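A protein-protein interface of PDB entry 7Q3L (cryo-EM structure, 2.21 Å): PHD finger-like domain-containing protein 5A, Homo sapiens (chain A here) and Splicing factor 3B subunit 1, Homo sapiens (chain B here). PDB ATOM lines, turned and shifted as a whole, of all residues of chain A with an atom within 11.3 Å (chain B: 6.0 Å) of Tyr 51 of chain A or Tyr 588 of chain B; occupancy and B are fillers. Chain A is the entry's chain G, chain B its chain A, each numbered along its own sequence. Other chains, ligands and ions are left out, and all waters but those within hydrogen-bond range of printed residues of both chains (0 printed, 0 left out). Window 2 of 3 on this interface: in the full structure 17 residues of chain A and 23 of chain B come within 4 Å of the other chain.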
ATOM      1  N   CYS A  11     -25.243 -26.567   5.791  1.00  0.00           N
ATOM      2  CA  CYS A  11     -24.229 -25.585   6.148  1.00  0.00           C
ATOM      3  C   CYS A  11     -24.817 -24.730   7.272  1.00  0.00           C
ATOM      4  O   CYS A  11     -26.027 -24.520   7.320  1.00  0.00           O
ATOM      5  CB  CYS A  11     -23.939 -24.744   4.908  1.00  0.00           C
ATOM      6  SG  CYS A  11     -22.678 -23.456   5.097  1.00  0.00           S
ATOM      7  N   LYS A  13     -22.603 -21.953   8.677  1.00  0.00           N
ATOM      8  CA  LYS A  13     -21.741 -20.780   8.741  1.00  0.00           C
ATOM      9  C   LYS A  13     -22.595 -19.516   8.772  1.00  0.00           C
ATOM     10  O   LYS A  13     -23.715 -19.494   8.263  1.00  0.00           O
ATOM     11  CB  LYS A  13     -20.804 -20.701   7.531  1.00  0.00           C
ATOM     12  CG  LYS A  13     -19.647 -21.692   7.549  1.00  0.00           C
ATOM     13  CD  LYS A  13     -18.486 -21.290   6.667  1.00  0.00           C
ATOM     14  CE  LYS A  13     -17.272 -22.176   6.857  1.00  0.00           C
ATOM     15  NZ  LYS A  13     -16.059 -21.589   6.241  1.00  0.00           N
ATOM     16  N   VAL A  17     -24.159 -11.249   2.579  1.00  0.00           N
ATOM     17  CA  VAL A  17     -24.939 -10.400   1.687  1.00  0.00           C
ATOM     18  C   VAL A  17     -25.558 -11.191   0.534  1.00  0.00           C
ATOM     19  O   VAL A  17     -26.598 -10.787   0.014  1.00  0.00           O
ATOM     20  CB  VAL A  17     -24.146  -9.177   1.186  1.00  0.00           C
ATOM     21  CG1 VAL A  17     -24.001  -8.155   2.295  1.00  0.00           C
ATOM     22  CG2 VAL A  17     -22.788  -9.548   0.606  1.00  0.00           C
ATOM     23  N   ALA A  18     -24.938 -12.318   0.151  1.00  0.00           N
ATOM     24  CA  ALA A  18     -25.394 -13.141  -0.962  1.00  0.00           C
ATOM     25  C   ALA A  18     -26.779 -13.734  -0.699  1.00  0.00           C
ATOM     26  O   ALA A  18     -27.046 -14.299   0.363  1.00  0.00           O
ATOM     27  CB  ALA A  18     -24.379 -14.215  -1.272  1.00  0.00           C
ATOM     28  N   ILE A  19     -27.650 -13.626  -1.710  1.00  0.00           N
ATOM     29  CA  ILE A  19     -29.016 -14.130  -1.661  1.00  0.00           C
ATOM     30  C   ILE A  19     -29.034 -15.580  -2.148  1.00  0.00           C
ATOM     31  O   ILE A  19     -28.362 -15.923  -3.119  1.00  0.00           O
ATOM     32  CB  ILE A  19     -29.955 -13.192  -2.455  1.00  0.00           C
ATOM     33  CG1 ILE A  19     -30.105 -11.851  -1.731  1.00  0.00           C
ATOM     34  CG2 ILE A  19     -31.314 -13.829  -2.740  1.00  0.00           C
ATOM     35  CD1 ILE A  19     -30.483 -10.692  -2.626  1.00  0.00           C
ATOM     36  N   GLY A  20     -29.799 -16.434  -1.455  1.00  0.00           N
ATOM     37  CA  GLY A  20     -29.957 -17.825  -1.845  1.00  0.00           C
ATOM     38  C   GLY A  20     -30.879 -17.960  -3.055  1.00  0.00           C
ATOM     39  O   GLY A  20     -31.809 -17.179  -3.217  1.00  0.00           O
ATOM     40  N   ARG A  21     -30.626 -18.977  -3.891  1.00  0.00           N
ATOM     41  CA  ARG A  21     -31.331 -19.179  -5.152  1.00  0.00           C
ATOM     42  C   ARG A  21     -31.993 -20.562  -5.206  1.00  0.00           C
ATOM     43  O   ARG A  21     -31.568 -21.484  -4.520  1.00  0.00           O
ATOM     44  CB  ARG A  21     -30.362 -18.972  -6.325  1.00  0.00           C
ATOM     45  CG  ARG A  21     -29.759 -17.575  -6.420  1.00  0.00           C
ATOM     46  CD  ARG A  21     -30.711 -16.494  -6.916  1.00  0.00           C
ATOM     47  NE  ARG A  21     -30.990 -16.668  -8.330  1.00  0.00           N
ATOM     48  CZ  ARG A  21     -31.880 -15.991  -9.050  1.00  0.00           C
ATOM     49  NH1 ARG A  21     -32.641 -15.048  -8.527  1.00  0.00           N
ATOM     50  NH2 ARG A  21     -32.024 -16.293 -10.323  1.00  0.00           N
ATOM     51  N   ILE A  45     -27.125 -16.615   2.004  1.00  0.00           N
ATOM     52  CA  ILE A  45     -26.169 -17.727   2.109  1.00  0.00           C
ATOM     53  C   ILE A  45     -24.752 -17.189   2.325  1.00  0.00           C
ATOM     54  O   ILE A  45     -24.512 -16.018   2.013  1.00  0.00           O
ATOM     55  CB  ILE A  45     -26.255 -18.682   0.898  1.00  0.00           C
ATOM     56  CG1 ILE A  45     -26.234 -17.941  -0.442  1.00  0.00           C
ATOM     57  CG2 ILE A  45     -27.459 -19.609   1.017  1.00  0.00           C
ATOM     58  CD1 ILE A  45     -26.419 -18.858  -1.623  1.00  0.00           C
ATOM     59  N   CYS A  46     -23.852 -18.022   2.876  1.00  0.00           N
ATOM     60  CA  CYS A  46     -22.476 -17.604   3.160  1.00  0.00           C
ATOM     61  C   CYS A  46     -21.695 -17.435   1.851  1.00  0.00           C
ATOM     62  O   CYS A  46     -22.061 -18.051   0.846  1.00  0.00           O
ATOM     63  CB  CYS A  46     -21.782 -18.579   4.114  1.00  0.00           C
ATOM     64  SG  CYS A  46     -21.325 -20.181   3.394  1.00  0.00           S
ATOM     65  N   ASP A  47     -20.628 -16.610   1.876  1.00  0.00           N
ATOM     66  CA  ASP A  47     -19.846 -16.306   0.681  1.00  0.00           C
ATOM     67  C   ASP A  47     -19.221 -17.558   0.059  1.00  0.00           C
ATOM     68  O   ASP A  47     -19.155 -17.662  -1.168  1.00  0.00           O
ATOM     69  CB  ASP A  47     -18.803 -15.221   0.953  1.00  0.00           C
ATOM     70  CG  ASP A  47     -19.340 -14.089   1.808  1.00  0.00           C
ATOM     71  OD1 ASP A  47     -19.246 -14.204   3.047  1.00  0.00           O
ATOM     72  OD2 ASP A  47     -19.845 -13.101   1.232  1.00  0.00           O
ATOM     73  N   GLU A  48     -18.751 -18.479   0.910  1.00  0.00           N
ATOM     74  CA  GLU A  48     -18.114 -19.709   0.450  1.00  0.00           C
ATOM     75  C   GLU A  48     -19.078 -20.534  -0.404  1.00  0.00           C
ATOM     76  O   GLU A  48     -18.677 -21.065  -1.448  1.00  0.00           O
ATOM     77  CB  GLU A  48     -17.594 -20.538   1.623  1.00  0.00           C
ATOM     78  CG  GLU A  48     -16.897 -19.708   2.679  1.00  0.00           C
ATOM     79  CD  GLU A  48     -15.389 -19.876   2.713  1.00  0.00           C
ATOM     80  OE1 GLU A  48     -14.911 -20.830   3.357  1.00  0.00           O
ATOM     81  OE2 GLU A  48     -14.700 -19.061   2.070  1.00  0.00           O
ATOM     82  N   CYS A  49     -20.348 -20.620   0.033  1.00  0.00           N
ATOM     83  CA  CYS A  49     -21.372 -21.384  -0.687  1.00  0.00           C
ATOM     84  C   CYS A  49     -21.819 -20.665  -1.968  1.00  0.00           C
ATOM     85  O   CYS A  49     -22.559 -21.268  -2.764  1.00  0.00           O
ATOM     86  CB  CYS A  49     -22.593 -21.642   0.200  1.00  0.00           C
ATOM     87  SG  CYS A  49     -22.274 -22.827   1.533  1.00  0.00           S
ATOM     88  N   ASN A  50     -21.417 -19.394  -2.138  1.00  0.00           N
ATOM     89  CA  ASN A  50     -21.803 -18.610  -3.322  1.00  0.00           C
ATOM     90  C   ASN A  50     -20.559 -18.139  -4.084  1.00  0.00           C
ATOM     91  O   ASN A  50     -20.558 -17.001  -4.577  1.00  0.00           O
ATOM     92  CB  ASN A  50     -22.713 -17.428  -2.959  1.00  0.00           C
ATOM     93  CG  ASN A  50     -23.970 -17.393  -3.807  1.00  0.00           C
ATOM     94  OD1 ASN A  50     -24.605 -16.356  -3.954  1.00  0.00           O
ATOM     95  ND2 ASN A  50     -24.342 -18.528  -4.355  1.00  0.00           N
ATOM     96  N   TYR A  51     -19.529 -18.989  -4.197  1.00  0.00           N
ATOM     97  CA  TYR A  51     -18.280 -18.574  -4.858  1.00  0.00           C
ATOM     98  C   TYR A  51     -17.991 -19.387  -6.125  1.00  0.00           C
ATOM     99  O   TYR A  51     -17.980 -20.612  -6.048  1.00  0.00           O
ATOM    100  CB  TYR A  51     -17.077 -18.683  -3.914  1.00  0.00           C
ATOM    101  CG  TYR A  51     -15.788 -18.181  -4.509  1.00  0.00           C
ATOM    102  CD1 TYR A  51     -15.519 -16.823  -4.571  1.00  0.00           C
ATOM    103  CD2 TYR A  51     -14.854 -19.057  -5.044  1.00  0.00           C
ATOM    104  CE1 TYR A  51     -14.342 -16.346  -5.122  1.00  0.00           C
ATOM    105  CE2 TYR A  51     -13.671 -18.598  -5.600  1.00  0.00           C
ATOM    106  CZ  TYR A  51     -13.418 -17.237  -5.639  1.00  0.00           C
ATOM    107  OH  TYR A  51     -12.261 -16.774  -6.186  1.00  0.00           O
ATOM    108  N   GLY A  52     -17.691 -18.719  -7.250  1.00  0.00           N
ATOM    109  CA  GLY A  52     -17.310 -19.428  -8.467  1.00  0.00           C
ATOM    110  C   GLY A  52     -18.429 -20.327  -8.998  1.00  0.00           C
ATOM    111  O   GLY A  52     -19.513 -19.830  -9.283  1.00  0.00           O
ATOM    112  N   SER A  53     -18.146 -21.632  -9.142  1.00  0.00           N
ATOM    113  CA  SER A  53     -19.158 -22.610  -9.522  1.00  0.00           C
ATOM    114  C   SER A  53     -20.303 -22.634  -8.509  1.00  0.00           C
ATOM    115  O   SER A  53     -21.468 -22.780  -8.886  1.00  0.00           O
ATOM    116  CB  SER A  53     -18.554 -23.981  -9.701  1.00  0.00           C
ATOM    117  OG  SER A  53     -17.365 -23.889 -10.466  1.00  0.00           O
ATOM    118  N   TYR A  54     -19.950 -22.484  -7.225  1.00  0.00           N
ATOM    119  CA  TYR A  54     -20.927 -22.490  -6.133  1.00  0.00           C
ATOM    120  C   TYR A  54     -21.893 -21.303  -6.268  1.00  0.00           C
ATOM    121  O   TYR A  54     -23.031 -21.402  -5.776  1.00  0.00           O
ATOM    122  CB  TYR A  54     -20.231 -22.501  -4.763  1.00  0.00           C
ATOM    123  CG  TYR A  54     -19.274 -23.643  -4.524  1.00  0.00           C
ATOM    124  CD1 TYR A  54     -19.380 -24.840  -5.218  1.00  0.00           C
ATOM    125  CD2 TYR A  54     -18.268 -23.531  -3.579  1.00  0.00           C
ATOM    126  CE1 TYR A  54     -18.503 -25.887  -4.995  1.00  0.00           C
ATOM    127  CE2 TYR A  54     -17.380 -24.569  -3.342  1.00  0.00           C
ATOM    128  CZ  TYR A  54     -17.499 -25.752  -4.050  1.00  0.00           C
ATOM    129  OH  TYR A  54     -16.632 -26.778  -3.819  1.00  0.00           O
ATOM    130  N   GLN A  55     -21.445 -20.186  -6.882  1.00  0.00           N
ATOM    131  CA  GLN A  55     -22.330 -19.027  -7.116  1.00  0.00           C
ATOM    132  C   GLN A  55     -23.523 -19.492  -7.949  1.00  0.00           C
ATOM    133  O   GLN A  55     -23.286 -20.135  -8.984  1.00  0.00           O
ATOM    134  CB  GLN A  55     -21.539 -17.861  -7.695  1.00  0.00           C
ATOM    135  CG  GLN A  55     -22.392 -16.721  -8.256  1.00  0.00           C
ATOM    136  CD  GLN A  55     -23.107 -15.983  -7.150  1.00  0.00           C
ATOM    137  OE1 GLN A  55     -24.335 -15.953  -7.074  1.00  0.00           O
ATOM    138  NE2 GLN A  55     -22.331 -15.339  -6.284  1.00  0.00           N
ATOM    139  N   GLY A  56     -24.755 -19.093  -7.576  1.00  0.00           N
ATOM    140  CA  GLY A  56     -25.947 -19.419  -8.347  1.00  0.00           C
ATOM    141  C   GLY A  56     -26.502 -20.820  -8.098  1.00  0.00           C
ATOM    142  O   GLY A  56     -27.466 -21.207  -8.767  1.00  0.00           O
ATOM    143  N   ARG A  57     -25.909 -21.562  -7.146  1.00  0.00           N
ATOM    144  CA  ARG A  57     -26.361 -22.918  -6.833  1.00  0.00           C
ATOM    145  C   ARG A  57     -27.735 -22.889  -6.159  1.00  0.00           C
ATOM    146  O   ARG A  57     -27.977 -22.001  -5.339  1.00  0.00           O
ATOM    147  CB  ARG A  57     -25.359 -23.637  -5.922  1.00  0.00           C
ATOM    148  CG  ARG A  57     -24.352 -24.499  -6.666  1.00  0.00           C
ATOM    149  CD  ARG A  57     -23.563 -25.372  -5.715  1.00  0.00           C
ATOM    150  NE  ARG A  57     -23.204 -24.666  -4.495  1.00  0.00           N
ATOM    151  CZ  ARG A  57     -22.513 -25.197  -3.492  1.00  0.00           C
ATOM    152  NH1 ARG A  57     -22.233 -24.472  -2.422  1.00  0.00           N
ATOM    153  NH2 ARG A  57     -22.102 -26.454  -3.549  1.00  0.00           N
ATOM    154  N   CYS A  58     -28.604 -23.863  -6.486  1.00  0.00           N
ATOM    155  CA  CYS A  58     -29.894 -23.975  -5.805  1.00  0.00           C
ATOM    156  C   CYS A  58     -29.607 -24.344  -4.351  1.00  0.00           C
ATOM    157  O   CYS A  58     -28.763 -25.214  -4.121  1.00  0.00           O
ATOM    158  CB  CYS A  58     -30.775 -25.022  -6.492  1.00  0.00           C
ATOM    159  SG  CYS A  58     -32.164 -25.664  -5.517  1.00  0.00           S
ATOM    160  N   GLY A  62     -28.465 -27.606  -5.444  1.00  0.00           N
ATOM    161  CA  GLY A  62     -27.226 -27.231  -6.124  1.00  0.00           C
ATOM    162  C   GLY A  62     -27.377 -27.027  -7.634  1.00  0.00           C
ATOM    163  O   GLY A  62     -26.356 -26.854  -8.312  1.00  0.00           O
ATOM    164  N   CYS A  85     -26.343 -20.049   7.243  1.00  0.00           N
ATOM    165  CA  CYS A  85     -26.448 -20.334   5.812  1.00  0.00           C
ATOM    166  C   CYS A  85     -27.106 -21.690   5.502  1.00  0.00           C
ATOM    167  O   CYS A  85     -26.423 -22.702   5.506  1.00  0.00           O
ATOM    168  CB  CYS A  85     -25.031 -20.302   5.246  1.00  0.00           C
ATOM    169  SG  CYS A  85     -24.840 -20.959   3.568  1.00  0.00           S
ATOM    170  N   LYS A  87     -27.621 -23.616   3.078  1.00  0.00           N
ATOM    171  CA  LYS A  87     -27.203 -24.404   1.925  1.00  0.00           C
ATOM    172  C   LYS A  87     -27.121 -25.871   2.345  1.00  0.00           C
ATOM    173  O   LYS A  87     -26.355 -26.193   3.249  1.00  0.00           O
ATOM    174  CB  LYS A  87     -25.845 -23.915   1.396  1.00  0.00           C
ATOM    175  CG  LYS A  87     -25.267 -24.714   0.229  1.00  0.00           C
ATOM    176  CD  LYS A  87     -25.959 -24.421  -1.103  1.00  0.00           C
ATOM    177  CE  LYS A  87     -25.798 -25.500  -2.161  1.00  0.00           C
ATOM    178  NZ  LYS A  87     -26.601 -26.709  -1.853  1.00  0.00           N
ATOM    179  N   ASP B 546     -11.596 -24.492 -11.288  1.00  0.00           N
ATOM    180  CA  ASP B 546     -11.794 -23.310 -10.452  1.00  0.00           C
ATOM    181  C   ASP B 546     -11.893 -23.652  -8.964  1.00  0.00           C
ATOM    182  O   ASP B 546     -11.277 -22.992  -8.129  1.00  0.00           O
ATOM    183  CB  ASP B 546     -13.017 -22.535 -10.929  1.00  0.00           C
ATOM    184  CG  ASP B 546     -12.767 -22.011 -12.323  1.00  0.00           C
ATOM    185  OD1 ASP B 546     -12.300 -20.878 -12.428  1.00  0.00           O
ATOM    186  OD2 ASP B 546     -12.954 -22.781 -13.280  1.00  0.00           O
ATOM    187  N   GLN B 547     -12.660 -24.695  -8.616  1.00  0.00           N
ATOM    188  CA  GLN B 547     -12.811 -25.064  -7.213  1.00  0.00           C
ATOM    189  C   GLN B 547     -11.552 -25.736  -6.658  1.00  0.00           C
ATOM    190  O   GLN B 547     -11.253 -25.579  -5.478  1.00  0.00           O
ATOM    191  CB  GLN B 547     -14.107 -25.847  -6.971  1.00  0.00           C
ATOM    192  CG  GLN B 547     -15.355 -25.258  -7.636  1.00  0.00           C
ATOM    193  CD  GLN B 547     -15.605 -23.783  -7.410  1.00  0.00           C
ATOM    194  OE1 GLN B 547     -15.441 -22.951  -8.304  1.00  0.00           O
ATOM    195  NE2 GLN B 547     -16.067 -23.445  -6.215  1.00  0.00           N
ATOM    196  N   ARG B 549      -8.414 -24.894  -7.749  1.00  0.00           N
ATOM    197  CA  ARG B 549      -7.618 -23.676  -7.647  1.00  0.00           C
ATOM    198  C   ARG B 549      -7.969 -22.875  -6.388  1.00  0.00           C
ATOM    199  O   ARG B 549      -7.067 -22.515  -5.636  1.00  0.00           O
ATOM    200  CB  ARG B 549      -7.787 -22.881  -8.946  1.00  0.00           C
ATOM    201  CG  ARG B 549      -6.801 -21.738  -9.156  1.00  0.00           C
ATOM    202  CD  ARG B 549      -7.180 -20.856 -10.361  1.00  0.00           C
ATOM    203  NE  ARG B 549      -8.488 -20.262 -10.101  1.00  0.00           N
ATOM    204  CZ  ARG B 549      -9.571 -20.240 -10.872  1.00  0.00           C
ATOM    205  NH1 ARG B 549      -9.567 -20.712 -12.109  1.00  0.00           N
ATOM    206  NH2 ARG B 549     -10.703 -19.780 -10.382  1.00  0.00           N
ATOM    207  N   HIS B 550      -9.263 -22.675  -6.109  1.00  0.00           N
ATOM    208  CA  HIS B 550      -9.770 -22.022  -4.901  1.00  0.00           C
ATOM    209  C   HIS B 550      -9.328 -22.728  -3.611  1.00  0.00           C
ATOM    210  O   HIS B 550      -8.858 -22.073  -2.680  1.00  0.00           O
ATOM    211  CB  HIS B 550     -11.293 -21.884  -5.031  1.00  0.00           C
ATOM    212  CG  HIS B 550     -12.036 -21.484  -3.802  1.00  0.00           C
ATOM    213  ND1 HIS B 550     -11.924 -20.230  -3.219  1.00  0.00           N
ATOM    214  CD2 HIS B 550     -12.970 -22.150  -3.093  1.00  0.00           C
ATOM    215  CE1 HIS B 550     -12.732 -20.164  -2.182  1.00  0.00           C
ATOM    216  NE2 HIS B 550     -13.380 -21.330  -2.084  1.00  0.00           N
ATOM    217  N   ASP B 586     -11.055 -14.800 -16.681  1.00  0.00           N
ATOM    218  CA  ASP B 586     -11.882 -15.320 -15.609  1.00  0.00           C
ATOM    219  C   ASP B 586     -11.754 -14.425 -14.372  1.00  0.00           C
ATOM    220  O   ASP B 586     -10.687 -14.355 -13.753  1.00  0.00           O
ATOM    221  CB  ASP B 586     -11.636 -16.819 -15.368  1.00  0.00           C
ATOM    222  CG  ASP B 586     -12.689 -17.296 -14.404  1.00  0.00           C
ATOM    223  OD1 ASP B 586     -12.518 -17.035 -13.197  1.00  0.00           O
ATOM    224  OD2 ASP B 586     -13.715 -17.829 -14.870  1.00  0.00           O
ATOM    225  N   TYR B 587     -12.891 -13.850 -13.954  1.00  0.00           N
ATOM    226  CA  TYR B 587     -13.003 -13.026 -12.754  1.00  0.00           C
ATOM    227  C   TYR B 587     -12.497 -13.729 -11.486  1.00  0.00           C
ATOM    228  O   TYR B 587     -11.866 -13.096 -10.637  1.00  0.00           O
ATOM    229  CB  TYR B 587     -14.451 -12.568 -12.540  1.00  0.00           C
ATOM    230  CG  TYR B 587     -14.576 -11.685 -11.320  1.00  0.00           C
ATOM    231  CD1 TYR B 587     -14.482 -10.299 -11.432  1.00  0.00           C
ATOM    232  CD2 TYR B 587     -14.690 -12.231 -10.047  1.00  0.00           C
ATOM    233  CE1 TYR B 587     -14.523  -9.478 -10.311  1.00  0.00           C
ATOM    234  CE2 TYR B 587     -14.729 -11.420  -8.920  1.00  0.00           C
ATOM    235  CZ  TYR B 587     -14.653 -10.039  -9.048  1.00  0.00           C
ATOM    236  OH  TYR B 587     -14.685  -9.218  -7.948  1.00  0.00           O
ATOM    237  N   TYR B 588     -12.787 -15.025 -11.338  1.00  0.00           N
ATOM    238  CA  TYR B 588     -12.427 -15.779 -10.145  1.00  0.00           C
ATOM    239  C   TYR B 588     -10.945 -16.156 -10.151  1.00  0.00           C
ATOM    240  O   TYR B 588     -10.265 -15.963  -9.148  1.00  0.00           O
ATOM    241  CB  TYR B 588     -13.397 -16.942  -9.952  1.00  0.00           C
ATOM    242  CG  TYR B 588     -14.827 -16.495  -9.791  1.00  0.00           C
ATOM    243  CD1 TYR B 588     -15.242 -15.787  -8.668  1.00  0.00           C
ATOM    244  CD2 TYR B 588     -15.771 -16.736 -10.782  1.00  0.00           C
ATOM    245  CE1 TYR B 588     -16.557 -15.352  -8.527  1.00  0.00           C
ATOM    246  CE2 TYR B 588     -17.092 -16.316 -10.650  1.00  0.00           C
ATOM    247  CZ  TYR B 588     -17.492 -15.620  -9.517  1.00  0.00           C
ATOM    248  OH  TYR B 588     -18.795 -15.201  -9.387  1.00  0.00           O
ATOM    249  N   ALA B 589     -10.402 -16.579 -11.301  1.00  0.00           N
ATOM    250  CA  ALA B 589      -8.959 -16.750 -11.465  1.00  0.00           C
ATOM    251  C   ALA B 589      -8.205 -15.446 -11.136  1.00  0.00           C
ATOM    252  O   ALA B 589      -7.162 -15.455 -10.474  1.00  0.00           O
ATOM    253  CB  ALA B 589      -8.667 -17.228 -12.868  1.00  0.00           C
ATOM    254  N   ARG B 590      -8.781 -14.311 -11.548  1.00  0.00           N
ATOM    255  CA  ARG B 590      -8.253 -12.977 -11.330  1.00  0.00           C
ATOM    256  C   ARG B 590      -8.261 -12.587  -9.848  1.00  0.00           C
ATOM    257  O   ARG B 590      -7.203 -12.270  -9.316  1.00  0.00           O
ATOM    258  CB  ARG B 590      -8.997 -12.022 -12.262  1.00  0.00           C
ATOM    259  CG  ARG B 590      -8.318 -10.675 -12.387  1.00  0.00           C
ATOM    260  CD  ARG B 590      -8.918 -10.002 -13.594  1.00  0.00           C
ATOM    261  NE  ARG B 590     -10.321  -9.636 -13.610  1.00  0.00           N
ATOM    262  CZ  ARG B 590     -11.244 -10.165 -14.415  1.00  0.00           C
ATOM    263  NH1 ARG B 590     -12.493  -9.737 -14.353  1.00  0.00           N
ATOM    264  NH2 ARG B 590     -10.943 -11.141 -15.254  1.00  0.00           N
ATOM    265  N   VAL B 591      -9.419 -12.644  -9.173  1.00  0.00           N
ATOM    266  CA  VAL B 591      -9.522 -12.304  -7.758  1.00  0.00           C
ATOM    267  C   VAL B 591      -8.636 -13.217  -6.904  1.00  0.00           C
ATOM    268  O   VAL B 591      -7.990 -12.744  -5.975  1.00  0.00           O
ATOM    269  CB  VAL B 591     -10.978 -12.239  -7.250  1.00  0.00           C
ATOM    270  CG1 VAL B 591     -11.615 -13.600  -7.011  1.00  0.00           C
ATOM    271  CG2 VAL B 591     -11.081 -11.419  -5.974  1.00  0.00           C
ATOM    272  N   GLU B 592      -8.546 -14.507  -7.248  1.00  0.00           N
ATOM    273  CA  GLU B 592      -7.658 -15.460  -6.592  1.00  0.00           C
ATOM    274  C   GLU B 592      -6.183 -15.069  -6.719  1.00  0.00           C
ATOM    275  O   GLU B 592      -5.453 -15.115  -5.735  1.00  0.00           O
ATOM    276  CB  GLU B 592      -7.910 -16.861  -7.130  1.00  0.00           C
ATOM    277  CG  GLU B 592      -9.167 -17.479  -6.552  1.00  0.00           C
ATOM    278  CD  GLU B 592      -9.652 -18.689  -7.328  1.00  0.00           C
ATOM    279  OE1 GLU B 592      -8.846 -19.616  -7.507  1.00  0.00           O
ATOM    280  OE2 GLU B 592     -10.808 -18.687  -7.800  1.00  0.00           O
ATOM    281  N   GLY B 593      -5.736 -14.642  -7.907  1.00  0.00           N
ATOM    282  CA  GLY B 593      -4.381 -14.133  -8.086  1.00  0.00           C
ATOM    283  C   GLY B 593      -4.089 -12.916  -7.201  1.00  0.00           C
ATOM    284  O   GLY B 593      -3.032 -12.840  -6.584  1.00  0.00           O
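O of Tyr 51 of chain A sits at hydrogen-bond distance from NE2 of Gln 547 of chain B, at 3.4 Å. The side-chain carboxylate of Glu 592 of chain B lies within hydrogen-bond range of the side-chain hydroxyl of Tyr 51 of chain A (2.9 Å). OG of Ser 53 of chain A lies within hydrogen-bond range of OE1 of Gln 547 of chain B (3.0 Å).
ND2 of Asn 50 of chain A lies within hydrogen-bond range of O of Tyr 54 of chain A, at 3.5 Å. NE of Arg 549 of chain B is in salt-bridge range of OE1 of Glu 592 of chain B (2.7 Å). N of His 550 of chain B is in hydrogen-bond range of OE1 of Glu 592 of chain B (3.4 Å). The side-chain carboxylate (OD1) of Asp 586 of chain B is in hydrogen-bond range of the backbone NH (N) of Tyr 588 of chain B (2.8 Å).
Among the printed residues, merely in contact across the chains: Tyr 51 of chain A with His 550 of chain B (3.4 Å), Tyr 51 of chain A with Tyr 588 of chain B (3.7 Å), Tyr 51 of chain A with Val 591 of chain B (3.3 Å), Gly 52 of chain A with Gln 547 of chain B (3.99 Å), Gly 52 of chain A with Tyr 588 of chain B (3.8 Å) and Tyr 54 of chain A with Gln 547 of chain B (3.4 Å).
Tyr 51 of chain A touches just these residues of chain B: Gln 547, His 550, Tyr 588, Val 591 and Glu 592. Tyr 588 of chain B touches two residues of chain A. His 550 of chain B touches one residue of chain A. No residue of chain A comes within 4 Å of Tyr 587 of chain B. No residue of chain A comes within 4 Å of Ala 589 of chain B. No residue of chain A comes within 4 Å of Arg 590 of chain B. Val 591 of chain B touches just one residue of chain A: Tyr 51 (3.3 Å). Of chain A, only Tyr 51 comes within 4 Å of Glu 592 of chain B. Of the printed residues of chain B, Tyr 54 of chain A touches Gln 547 (3.4 Å). Of the printed residues of chain B, Ser 53 of chain A touches Gln 547. Printed residues of chain B within 4 Å of Gly 52 of chain A: Gln 547 (3.99 Å) and Tyr 588 (3.8 Å). Of the printed residues of chain A, Gln 547 of chain B touches Tyr 51, Gly 52, Ser 53 and Tyr 54. Lys 87 of chain A touches none of the printed residues of chain B. The nearest residue of chain B that does not touch Tyr 51 of chain A is Arg 549 of chain B (5.4 Å).
Of the 24 printed residues of chain A, 4 touch a printed residue of chain B. Hydrophobic or aromatic side chains of chain A within 4 Å of the printed part of chain B: Tyr 51 and Tyr 54. Along chain B the printed residues that touch a printed residue of chain A span positions 547 to 592.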
